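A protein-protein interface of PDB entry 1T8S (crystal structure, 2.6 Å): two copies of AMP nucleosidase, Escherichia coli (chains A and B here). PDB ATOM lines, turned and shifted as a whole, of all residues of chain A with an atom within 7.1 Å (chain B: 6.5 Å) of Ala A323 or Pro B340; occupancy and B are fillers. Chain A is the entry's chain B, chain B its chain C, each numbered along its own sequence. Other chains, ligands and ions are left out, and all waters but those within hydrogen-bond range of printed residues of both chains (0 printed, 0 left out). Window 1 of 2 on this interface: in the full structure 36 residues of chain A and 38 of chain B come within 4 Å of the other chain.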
ATOM      1  N   LEU A 320      28.515  27.899 -18.043  1.00  0.00           N
ATOM      2  CA  LEU A 320      29.452  27.144 -18.869  1.00  0.00           C
ATOM      3  C   LEU A 320      29.017  25.673 -18.725  1.00  0.00           C
ATOM      4  O   LEU A 320      29.090  25.103 -17.628  1.00  0.00           O
ATOM      5  CB  LEU A 320      30.876  27.316 -18.350  1.00  0.00           C
ATOM      6  CG  LEU A 320      31.921  26.399 -18.997  1.00  0.00           C
ATOM      7  CD1 LEU A 320      32.055  26.740 -20.467  1.00  0.00           C
ATOM      8  CD2 LEU A 320      33.248  26.541 -18.290  1.00  0.00           C
ATOM      9  N   ALA A 321      28.560  25.070 -19.818  1.00  0.00           N
ATOM     10  CA  ALA A 321      28.072  23.693 -19.775  1.00  0.00           C
ATOM     11  C   ALA A 321      29.167  22.657 -19.682  1.00  0.00           C
ATOM     12  O   ALA A 321      30.056  22.636 -20.526  1.00  0.00           O
ATOM     13  CB  ALA A 321      27.217  23.409 -20.997  1.00  0.00           C
ATOM     14  N   HIS A 322      29.117  21.807 -18.654  1.00  0.00           N
ATOM     15  CA  HIS A 322      30.107  20.738 -18.522  1.00  0.00           C
ATOM     16  C   HIS A 322      29.444  19.415 -18.901  1.00  0.00           C
ATOM     17  O   HIS A 322      30.085  18.365 -18.902  1.00  0.00           O
ATOM     18  CB  HIS A 322      30.695  20.646 -17.094  1.00  0.00           C
ATOM     19  CG  HIS A 322      29.740  20.155 -16.043  1.00  0.00           C
ATOM     20  ND1 HIS A 322      28.428  19.810 -16.306  1.00  0.00           N
ATOM     21  CD2 HIS A 322      29.909  19.973 -14.709  1.00  0.00           C
ATOM     22  CE1 HIS A 322      27.833  19.439 -15.183  1.00  0.00           C
ATOM     23  NE2 HIS A 322      28.709  19.529 -14.200  1.00  0.00           N
ATOM     24  N   ALA A 323      28.154  19.471 -19.218  1.00  0.00           N
ATOM     25  CA  ALA A 323      27.401  18.285 -19.600  1.00  0.00           C
ATOM     26  C   ALA A 323      26.022  18.713 -20.087  1.00  0.00           C
ATOM     27  O   ALA A 323      25.584  19.836 -19.829  1.00  0.00           O
ATOM     28  CB  ALA A 323      27.267  17.332 -18.412  1.00  0.00           C
ATOM     29  N   TYR A 324      25.333  17.804 -20.765  1.00  0.00           N
ATOM     30  CA  TYR A 324      24.018  18.103 -21.290  1.00  0.00           C
ATOM     31  C   TYR A 324      22.981  17.018 -21.015  1.00  0.00           C
ATOM     32  O   TYR A 324      23.265  15.828 -21.136  1.00  0.00           O
ATOM     33  CB  TYR A 324      24.111  18.272 -22.803  1.00  0.00           C
ATOM     34  CG  TYR A 324      25.147  19.252 -23.265  1.00  0.00           C
ATOM     35  CD1 TYR A 324      24.827  20.606 -23.444  1.00  0.00           C
ATOM     36  CD2 TYR A 324      26.445  18.838 -23.531  1.00  0.00           C
ATOM     37  CE1 TYR A 324      25.783  21.519 -23.882  1.00  0.00           C
ATOM     38  CE2 TYR A 324      27.414  19.747 -23.973  1.00  0.00           C
ATOM     39  CZ  TYR A 324      27.074  21.083 -24.143  1.00  0.00           C
ATOM     40  OH  TYR A 324      28.037  21.975 -24.556  1.00  0.00           O
ATOM     41  N   LEU A 325      21.775  17.437 -20.652  1.00  0.00           N
ATOM     42  CA  LEU A 325      20.679  16.504 -20.454  1.00  0.00           C
ATOM     43  C   LEU A 325      19.940  16.640 -21.789  1.00  0.00           C
ATOM     44  O   LEU A 325      19.210  17.616 -22.007  1.00  0.00           O
ATOM     45  CB  LEU A 325      19.753  16.939 -19.312  1.00  0.00           C
ATOM     46  CG  LEU A 325      18.541  16.004 -19.151  1.00  0.00           C
ATOM     47  CD1 LEU A 325      19.008  14.568 -18.880  1.00  0.00           C
ATOM     48  CD2 LEU A 325      17.675  16.479 -18.008  1.00  0.00           C
ATOM     49  N   ARG A 326      20.158  15.683 -22.689  1.00  0.00           N
ATOM     50  CA  ARG A 326      19.531  15.710 -24.011  1.00  0.00           C
ATOM     51  C   ARG A 326      18.032  15.370 -24.080  1.00  0.00           C
ATOM     52  O   ARG A 326      17.671  14.225 -24.314  1.00  0.00           O
ATOM     53  CB  ARG A 326      20.307  14.784 -24.947  1.00  0.00           C
ATOM     54  CG  ARG A 326      21.647  15.331 -25.342  1.00  0.00           C
ATOM     55  CD  ARG A 326      22.738  14.278 -25.470  1.00  0.00           C
ATOM     56  NE  ARG A 326      22.484  13.209 -26.443  1.00  0.00           N
ATOM     57  CZ  ARG A 326      21.927  13.382 -27.640  1.00  0.00           C
ATOM     58  NH1 ARG A 326      21.539  14.593 -28.030  1.00  0.00           N
ATOM     59  NH2 ARG A 326      21.779  12.356 -28.467  1.00  0.00           N
ATOM     60  N   PRO A 337      20.405   8.777 -26.304  1.00  0.00           N
ATOM     61  CA  PRO A 337      20.580   9.652 -25.138  1.00  0.00           C
ATOM     62  C   PRO A 337      21.523   9.165 -24.045  1.00  0.00           C
ATOM     63  O   PRO A 337      21.956   9.954 -23.218  1.00  0.00           O
ATOM     64  CB  PRO A 337      19.153   9.835 -24.609  1.00  0.00           C
ATOM     65  CG  PRO A 337      18.293   9.566 -25.788  1.00  0.00           C
ATOM     66  CD  PRO A 337      18.992   8.397 -26.449  1.00  0.00           C
ATOM     67  N   PRO A 340      27.302   9.258 -23.617  1.00  0.00           N
ATOM     68  CA  PRO A 340      27.764  10.507 -23.021  1.00  0.00           C
ATOM     69  C   PRO A 340      28.468  11.494 -23.955  1.00  0.00           C
ATOM     70  O   PRO A 340      29.437  11.135 -24.628  1.00  0.00           O
ATOM     71  CB  PRO A 340      28.691  10.014 -21.910  1.00  0.00           C
ATOM     72  CG  PRO A 340      29.340   8.817 -22.548  1.00  0.00           C
ATOM     73  CD  PRO A 340      28.165   8.128 -23.222  1.00  0.00           C
ATOM     74  N   ILE A 341      27.981  12.735 -23.979  1.00  0.00           N
ATOM     75  CA  ILE A 341      28.600  13.806 -24.769  1.00  0.00           C
ATOM     76  C   ILE A 341      29.476  14.599 -23.779  1.00  0.00           C
ATOM     77  O   ILE A 341      28.962  15.372 -22.972  1.00  0.00           O
ATOM     78  CB  ILE A 341      27.554  14.780 -25.339  1.00  0.00           C
ATOM     79  CG1 ILE A 341      26.500  14.016 -26.137  1.00  0.00           C
ATOM     80  CG2 ILE A 341      28.247  15.855 -26.155  1.00  0.00           C
ATOM     81  CD1 ILE A 341      27.040  13.237 -27.300  1.00  0.00           C
ATOM     82  N   PRO A 342      30.798  14.417 -23.831  1.00  0.00           N
ATOM     83  CA  PRO A 342      31.748  15.100 -22.943  1.00  0.00           C
ATOM     84  C   PRO A 342      32.088  16.551 -23.303  1.00  0.00           C
ATOM     85  O   PRO A 342      31.657  17.073 -24.334  1.00  0.00           O
ATOM     86  CB  PRO A 342      32.983  14.211 -23.026  1.00  0.00           C
ATOM     87  CG  PRO A 342      32.987  13.834 -24.482  1.00  0.00           C
ATOM     88  CD  PRO A 342      31.506  13.556 -24.799  1.00  0.00           C
ATOM     89  N   SER A 343      32.880  17.184 -22.441  1.00  0.00           N
ATOM     90  CA  SER A 343      33.325  18.563 -22.636  1.00  0.00           C
ATOM     91  C   SER A 343      34.725  18.500 -23.191  1.00  0.00           C
ATOM     92  O   SER A 343      35.493  17.614 -22.830  1.00  0.00           O
ATOM     93  CB  SER A 343      33.394  19.326 -21.312  1.00  0.00           C
ATOM     94  OG  SER A 343      32.129  19.409 -20.680  1.00  0.00           O
ATOM     95  N   GLN A 348      36.773  24.408 -22.970  1.00  0.00           N
ATOM     96  CA  GLN A 348      36.254  24.797 -21.671  1.00  0.00           C
ATOM     97  C   GLN A 348      37.153  25.832 -20.999  1.00  0.00           C
ATOM     98  O   GLN A 348      36.653  26.797 -20.428  1.00  0.00           O
ATOM     99  CB  GLN A 348      36.098  23.561 -20.790  1.00  0.00           C
ATOM    100  CG  GLN A 348      35.122  22.558 -21.369  1.00  0.00           C
ATOM    101  CD  GLN A 348      33.679  22.999 -21.260  1.00  0.00           C
ATOM    102  OE1 GLN A 348      33.108  22.995 -20.175  1.00  0.00           O
ATOM    103  NE2 GLN A 348      33.082  23.383 -22.381  1.00  0.00           N
ATOM    104  N   THR A 372      29.311  26.732 -13.576  1.00  0.00           N
ATOM    105  CA  THR A 372      29.658  25.641 -14.487  1.00  0.00           C
ATOM    106  C   THR A 372      28.787  24.448 -14.110  1.00  0.00           C
ATOM    107  O   THR A 372      28.802  24.006 -12.962  1.00  0.00           O
ATOM    108  CB  THR A 372      31.112  25.236 -14.346  1.00  0.00           C
ATOM    109  OG1 THR A 372      31.944  26.249 -14.925  1.00  0.00           O
ATOM    110  CG2 THR A 372      31.363  23.903 -15.047  1.00  0.00           C
ATOM    111  N   GLY A 373      28.017  23.933 -15.061  1.00  0.00           N
ATOM    112  CA  GLY A 373      27.147  22.819 -14.739  1.00  0.00           C
ATOM    113  C   GLY A 373      26.422  22.209 -15.914  1.00  0.00           C
ATOM    114  O   GLY A 373      26.741  22.481 -17.074  1.00  0.00           O
ATOM    115  N   THR A 374      25.435  21.375 -15.604  1.00  0.00           N
ATOM    116  CA  THR A 374      24.663  20.691 -16.618  1.00  0.00           C
ATOM    117  C   THR A 374      23.534  21.545 -17.152  1.00  0.00           C
ATOM    118  O   THR A 374      22.802  22.194 -16.386  1.00  0.00           O
ATOM    119  CB  THR A 374      24.108  19.357 -16.073  1.00  0.00           C
ATOM    120  OG1 THR A 374      25.198  18.448 -15.887  1.00  0.00           O
ATOM    121  CG2 THR A 374      23.104  18.724 -17.064  1.00  0.00           C
ATOM    122  N   VAL A 375      23.407  21.536 -18.476  1.00  0.00           N
ATOM    123  CA  VAL A 375      22.381  22.283 -19.181  1.00  0.00           C
ATOM    124  C   VAL A 375      21.361  21.319 -19.784  1.00  0.00           C
ATOM    125  O   VAL A 375      21.712  20.289 -20.344  1.00  0.00           O
ATOM    126  CB  VAL A 375      23.004  23.121 -20.349  1.00  0.00           C
ATOM    127  CG1 VAL A 375      21.907  23.797 -21.182  1.00  0.00           C
ATOM    128  CG2 VAL A 375      23.964  24.164 -19.797  1.00  0.00           C
ATOM    129  N   VAL A 376      20.091  21.662 -19.680  1.00  0.00           N
ATOM    130  CA  VAL A 376      19.042  20.837 -20.242  1.00  0.00           C
ATOM    131  C   VAL A 376      18.622  21.465 -21.566  1.00  0.00           C
ATOM    132  O   VAL A 376      18.284  22.636 -21.619  1.00  0.00           O
ATOM    133  CB  VAL A 376      17.784  20.819 -19.350  1.00  0.00           C
ATOM    134  CG1 VAL A 376      16.733  19.888 -19.944  1.00  0.00           C
ATOM    135  CG2 VAL A 376      18.138  20.419 -17.961  1.00  0.00           C
ATOM    136  N   LEU A 396      17.546  15.287 -10.980  1.00  0.00           N
ATOM    137  CA  LEU A 396      18.394  14.135 -11.222  1.00  0.00           C
ATOM    138  C   LEU A 396      19.669  14.529 -11.943  1.00  0.00           C
ATOM    139  O   LEU A 396      20.739  13.978 -11.669  1.00  0.00           O
ATOM    140  CB  LEU A 396      17.633  13.108 -12.058  1.00  0.00           C
ATOM    141  CG  LEU A 396      17.399  11.715 -11.479  1.00  0.00           C
ATOM    142  CD1 LEU A 396      17.346  11.757  -9.955  1.00  0.00           C
ATOM    143  CD2 LEU A 396      16.109  11.178 -12.069  1.00  0.00           C
ATOM    144  N   SER A 397      19.562  15.479 -12.870  1.00  0.00           N
ATOM    145  CA  SER A 397      20.737  15.919 -13.626  1.00  0.00           C
ATOM    146  C   SER A 397      21.469  17.124 -13.028  1.00  0.00           C
ATOM    147  O   SER A 397      22.461  17.586 -13.596  1.00  0.00           O
ATOM    148  CB  SER A 397      20.355  16.235 -15.069  1.00  0.00           C
ATOM    149  OG  SER A 397      19.507  17.369 -15.136  1.00  0.00           O
ATOM    150  N   ARG A 398      20.998  17.622 -11.886  1.00  0.00           N
ATOM    151  CA  ARG A 398      21.630  18.777 -11.235  1.00  0.00           C
ATOM    152  C   ARG A 398      21.658  19.925 -12.242  1.00  0.00           C
ATOM    153  O   ARG A 398      22.608  20.706 -12.300  1.00  0.00           O
ATOM    154  CB  ARG A 398      23.065  18.431 -10.810  1.00  0.00           C
ATOM    155  CG  ARG A 398      23.228  17.104 -10.075  1.00  0.00           C
ATOM    156  CD  ARG A 398      22.594  17.125  -8.694  1.00  0.00           C
ATOM    157  NE  ARG A 398      22.986  15.960  -7.902  1.00  0.00           N
ATOM    158  CZ  ARG A 398      22.418  14.756  -7.967  1.00  0.00           C
ATOM    159  NH1 ARG A 398      21.401  14.526  -8.788  1.00  0.00           N
ATOM    160  NH2 ARG A 398      22.882  13.777  -7.204  1.00  0.00           N
ATOM    161  N   ALA A 407      22.636  21.237 -26.404  1.00  0.00           N
ATOM    162  CA  ALA A 407      22.921  19.812 -26.516  1.00  0.00           C
ATOM    163  C   ALA A 407      22.966  19.358 -27.968  1.00  0.00           C
ATOM    164  O   ALA A 407      23.783  18.500 -28.335  1.00  0.00           O
ATOM    165  CB  ALA A 407      21.887  19.002 -25.734  1.00  0.00           C
ATOM    166  N   ARG B 326      27.674   4.066 -19.088  1.00  0.00           N
ATOM    167  CA  ARG B 326      27.099   3.230 -18.034  1.00  0.00           C
ATOM    168  C   ARG B 326      26.387   1.956 -18.478  1.00  0.00           C
ATOM    169  O   ARG B 326      25.177   1.949 -18.609  1.00  0.00           O
ATOM    170  CB  ARG B 326      26.135   4.083 -17.183  1.00  0.00           C
ATOM    171  CG  ARG B 326      26.847   5.079 -16.292  1.00  0.00           C
ATOM    172  CD  ARG B 326      26.131   6.408 -16.134  1.00  0.00           C
ATOM    173  NE  ARG B 326      24.802   6.341 -15.512  1.00  0.00           N
ATOM    174  CZ  ARG B 326      24.489   5.558 -14.488  1.00  0.00           C
ATOM    175  NH1 ARG B 326      25.403   4.750 -13.959  1.00  0.00           N
ATOM    176  NH2 ARG B 326      23.270   5.594 -13.985  1.00  0.00           N
ATOM    177  N   PRO B 336      18.715   7.105 -14.179  1.00  0.00           N
ATOM    178  CA  PRO B 336      18.656   6.655 -15.577  1.00  0.00           C
ATOM    179  C   PRO B 336      19.949   6.888 -16.362  1.00  0.00           C
ATOM    180  O   PRO B 336      20.624   7.893 -16.181  1.00  0.00           O
ATOM    181  CB  PRO B 336      17.464   7.425 -16.128  1.00  0.00           C
ATOM    182  CG  PRO B 336      16.547   7.480 -14.945  1.00  0.00           C
ATOM    183  CD  PRO B 336      17.507   7.872 -13.825  1.00  0.00           C
ATOM    184  N   PRO B 337      20.293   5.956 -17.267  1.00  0.00           N
ATOM    185  CA  PRO B 337      21.508   6.026 -18.083  1.00  0.00           C
ATOM    186  C   PRO B 337      21.688   7.280 -18.920  1.00  0.00           C
ATOM    187  O   PRO B 337      22.807   7.573 -19.352  1.00  0.00           O
ATOM    188  CB  PRO B 337      21.422   4.778 -18.960  1.00  0.00           C
ATOM    189  CG  PRO B 337      20.468   3.878 -18.218  1.00  0.00           C
ATOM    190  CD  PRO B 337      19.444   4.838 -17.706  1.00  0.00           C
ATOM    191  N   ASP B 338      20.614   8.016 -19.171  1.00  0.00           N
ATOM    192  CA  ASP B 338      20.763   9.221 -19.978  1.00  0.00           C
ATOM    193  C   ASP B 338      21.078  10.454 -19.142  1.00  0.00           C
ATOM    194  O   ASP B 338      21.296  11.525 -19.710  1.00  0.00           O
ATOM    195  CB  ASP B 338      19.514   9.472 -20.808  1.00  0.00           C
ATOM    196  CG  ASP B 338      18.309   9.641 -19.963  1.00  0.00           C
ATOM    197  OD1 ASP B 338      18.040   8.750 -19.133  1.00  0.00           O
ATOM    198  OD2 ASP B 338      17.623  10.661 -20.123  1.00  0.00           O
ATOM    199  N   ILE B 339      21.093  10.318 -17.813  1.00  0.00           N
ATOM    200  CA  ILE B 339      21.432  11.451 -16.953  1.00  0.00           C
ATOM    201  C   ILE B 339      22.951  11.522 -17.062  1.00  0.00           C
ATOM    202  O   ILE B 339      23.640  10.582 -16.714  1.00  0.00           O
ATOM    203  CB  ILE B 339      21.050  11.221 -15.460  1.00  0.00           C
ATOM    204  CG1 ILE B 339      19.558  10.916 -15.313  1.00  0.00           C
ATOM    205  CG2 ILE B 339      21.348  12.460 -14.658  1.00  0.00           C
ATOM    206  CD1 ILE B 339      18.648  12.020 -15.765  1.00  0.00           C
ATOM    207  N   PRO B 340      23.493  12.638 -17.556  1.00  0.00           N
ATOM    208  CA  PRO B 340      24.952  12.729 -17.679  1.00  0.00           C
ATOM    209  C   PRO B 340      25.706  12.828 -16.361  1.00  0.00           C
ATOM    210  O   PRO B 340      25.333  13.603 -15.486  1.00  0.00           O
ATOM    211  CB  PRO B 340      25.148  13.977 -18.540  1.00  0.00           C
ATOM    212  CG  PRO B 340      24.018  14.861 -18.082  1.00  0.00           C
ATOM    213  CD  PRO B 340      22.838  13.891 -17.979  1.00  0.00           C
ATOM    214  N   ILE B 341      26.753  12.024 -16.233  1.00  0.00           N
ATOM    215  CA  ILE B 341      27.616  12.024 -15.061  1.00  0.00           C
ATOM    216  C   ILE B 341      28.880  12.772 -15.476  1.00  0.00           C
ATOM    217  O   ILE B 341      29.752  12.222 -16.133  1.00  0.00           O
ATOM    218  CB  ILE B 341      28.029  10.598 -14.642  1.00  0.00           C
ATOM    219  CG1 ILE B 341      26.780   9.757 -14.361  1.00  0.00           C
ATOM    220  CG2 ILE B 341      28.938  10.665 -13.407  1.00  0.00           C
ATOM    221  CD1 ILE B 341      25.880  10.336 -13.277  1.00  0.00           C
ATOM    222  N   PRO B 342      29.007  14.033 -15.073  1.00  0.00           N
ATOM    223  CA  PRO B 342      30.181  14.829 -15.439  1.00  0.00           C
ATOM    224  C   PRO B 342      31.462  14.538 -14.660  1.00  0.00           C
ATOM    225  O   PRO B 342      31.480  13.734 -13.733  1.00  0.00           O
ATOM    226  CB  PRO B 342      29.694  16.244 -15.198  1.00  0.00           C
ATOM    227  CG  PRO B 342      28.918  16.058 -13.904  1.00  0.00           C
ATOM    228  CD  PRO B 342      28.114  14.791 -14.174  1.00  0.00           C
ATOM    229  N   TYR B 414      28.406  11.130  -7.497  1.00  0.00           N
ATOM    230  CA  TYR B 414      27.511  12.146  -8.026  1.00  0.00           C
ATOM    231  C   TYR B 414      26.232  12.126  -7.195  1.00  0.00           C
ATOM    232  O   TYR B 414      25.773  13.162  -6.719  1.00  0.00           O
ATOM    233  CB  TYR B 414      27.226  11.826  -9.490  1.00  0.00           C
ATOM    234  CG  TYR B 414      26.152  12.630 -10.181  1.00  0.00           C
ATOM    235  CD1 TYR B 414      26.485  13.714 -10.990  1.00  0.00           C
ATOM    236  CD2 TYR B 414      24.804  12.274 -10.063  1.00  0.00           C
ATOM    237  CE1 TYR B 414      25.505  14.433 -11.681  1.00  0.00           C
ATOM    238  CE2 TYR B 414      23.815  12.981 -10.734  1.00  0.00           C
ATOM    239  CZ  TYR B 414      24.169  14.068 -11.549  1.00  0.00           C
ATOM    240  OH  TYR B 414      23.177  14.784 -12.189  1.00  0.00           O
ATOM    241  N   TYR B 420      34.423  12.921  -7.008  1.00  0.00           N
ATOM    242  CA  TYR B 420      34.968  11.642  -7.453  1.00  0.00           C
ATOM    243  C   TYR B 420      35.874  11.782  -8.651  1.00  0.00           C
ATOM    244  O   TYR B 420      35.837  12.780  -9.358  1.00  0.00           O
ATOM    245  CB  TYR B 420      33.799  10.712  -7.817  1.00  0.00           C
ATOM    246  CG  TYR B 420      32.816  11.376  -8.773  1.00  0.00           C
ATOM    247  CD1 TYR B 420      33.021  11.337 -10.155  1.00  0.00           C
ATOM    248  CD2 TYR B 420      31.719  12.110  -8.292  1.00  0.00           C
ATOM    249  CE1 TYR B 420      32.174  12.006 -11.030  1.00  0.00           C
ATOM    250  CE2 TYR B 420      30.863  12.785  -9.171  1.00  0.00           C
ATOM    251  CZ  TYR B 420      31.106  12.723 -10.534  1.00  0.00           C
ATOM    252  OH  TYR B 420      30.267  13.363 -11.405  1.00  0.00           O
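The backbone carbonyl oxygen of Leu A396 is in hydrogen-bond range of the side-chain hydroxyl of Tyr B414 (2.6 Å). OH of Tyr B414 sits close to O of Ser A397 (3.2 Å). The guanidinium group (NH2) of Arg A398 sits at hydrogen-bond distance from the backbone carbonyl oxygen (O) of Tyr B414.
The backbone carbonyl oxygen (O) of His A322 lies within hydrogen-bond range of the side-chain hydroxyl (OG) of Ser A343. The backbone NH of Thr A374 sits close to a ring nitrogen (ND1) of His A322 (3.4 Å). The backbone carbonyl oxygen (O) of Ala A323 is in hydrogen-bond range of the backbone NH (N) of Val A375, 3.1 Å away. The backbone NH (N) of Leu A325 lies within hydrogen-bond range of the backbone carbonyl oxygen (O) of Val A375 (2.9 Å). O of Leu A396 is in hydrogen-bond range of NH1 of Arg A398, at 3.0 Å. The side-chain hydroxyl (OH) of Tyr B420 is in hydrogen-bond range of the backbone carbonyl oxygen (O) of Pro B342, at 2.7 Å.
Among the printed residues, merely in contact across the chains: His A322 with Pro B342, Ala A323 with Pro B340, Tyr A324 with Pro B340, Leu A325 with Asp B338, Leu A325 with Pro B340, Pro A337 with Asp B338, Leu A396 with Pro B336, Leu A396 with Ile B339 and Ser A397 with Ile B339.
Ala A323 touches just one residue of chain B: Pro B340. Printed residues of chain A within 4 Å of Pro B340: Ala A323, Tyr A324 and Leu A325. Of the printed residues of chain B, His A322 touches Pro B342. Of the printed residues of chain A, Tyr B414 touches Leu A396, Ser A397 and Arg A398. Gln A348 touches none of the printed residues of chain B. The nearest printed residue of chain A that does not touch Pro B340 is Thr A374 (4.1 Å).
Hydrophobic or aromatic side chains of chain B within 4 Å of the printed part of chain A: Pro B336, Ile B339, Pro B340, Pro B342 and Tyr B414. Among the printed residues, 12 pairs touch across the chains. Among the printed residues, no Asp or Glu carboxylate lies within 4 Å of a Lys or Arg side-chain nitrogen of the other chain.
5 positions are printed for both chains. Of the 12 pairs that touch across the chains among the printed residues, none has its exchanged pair printed and touching as well.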
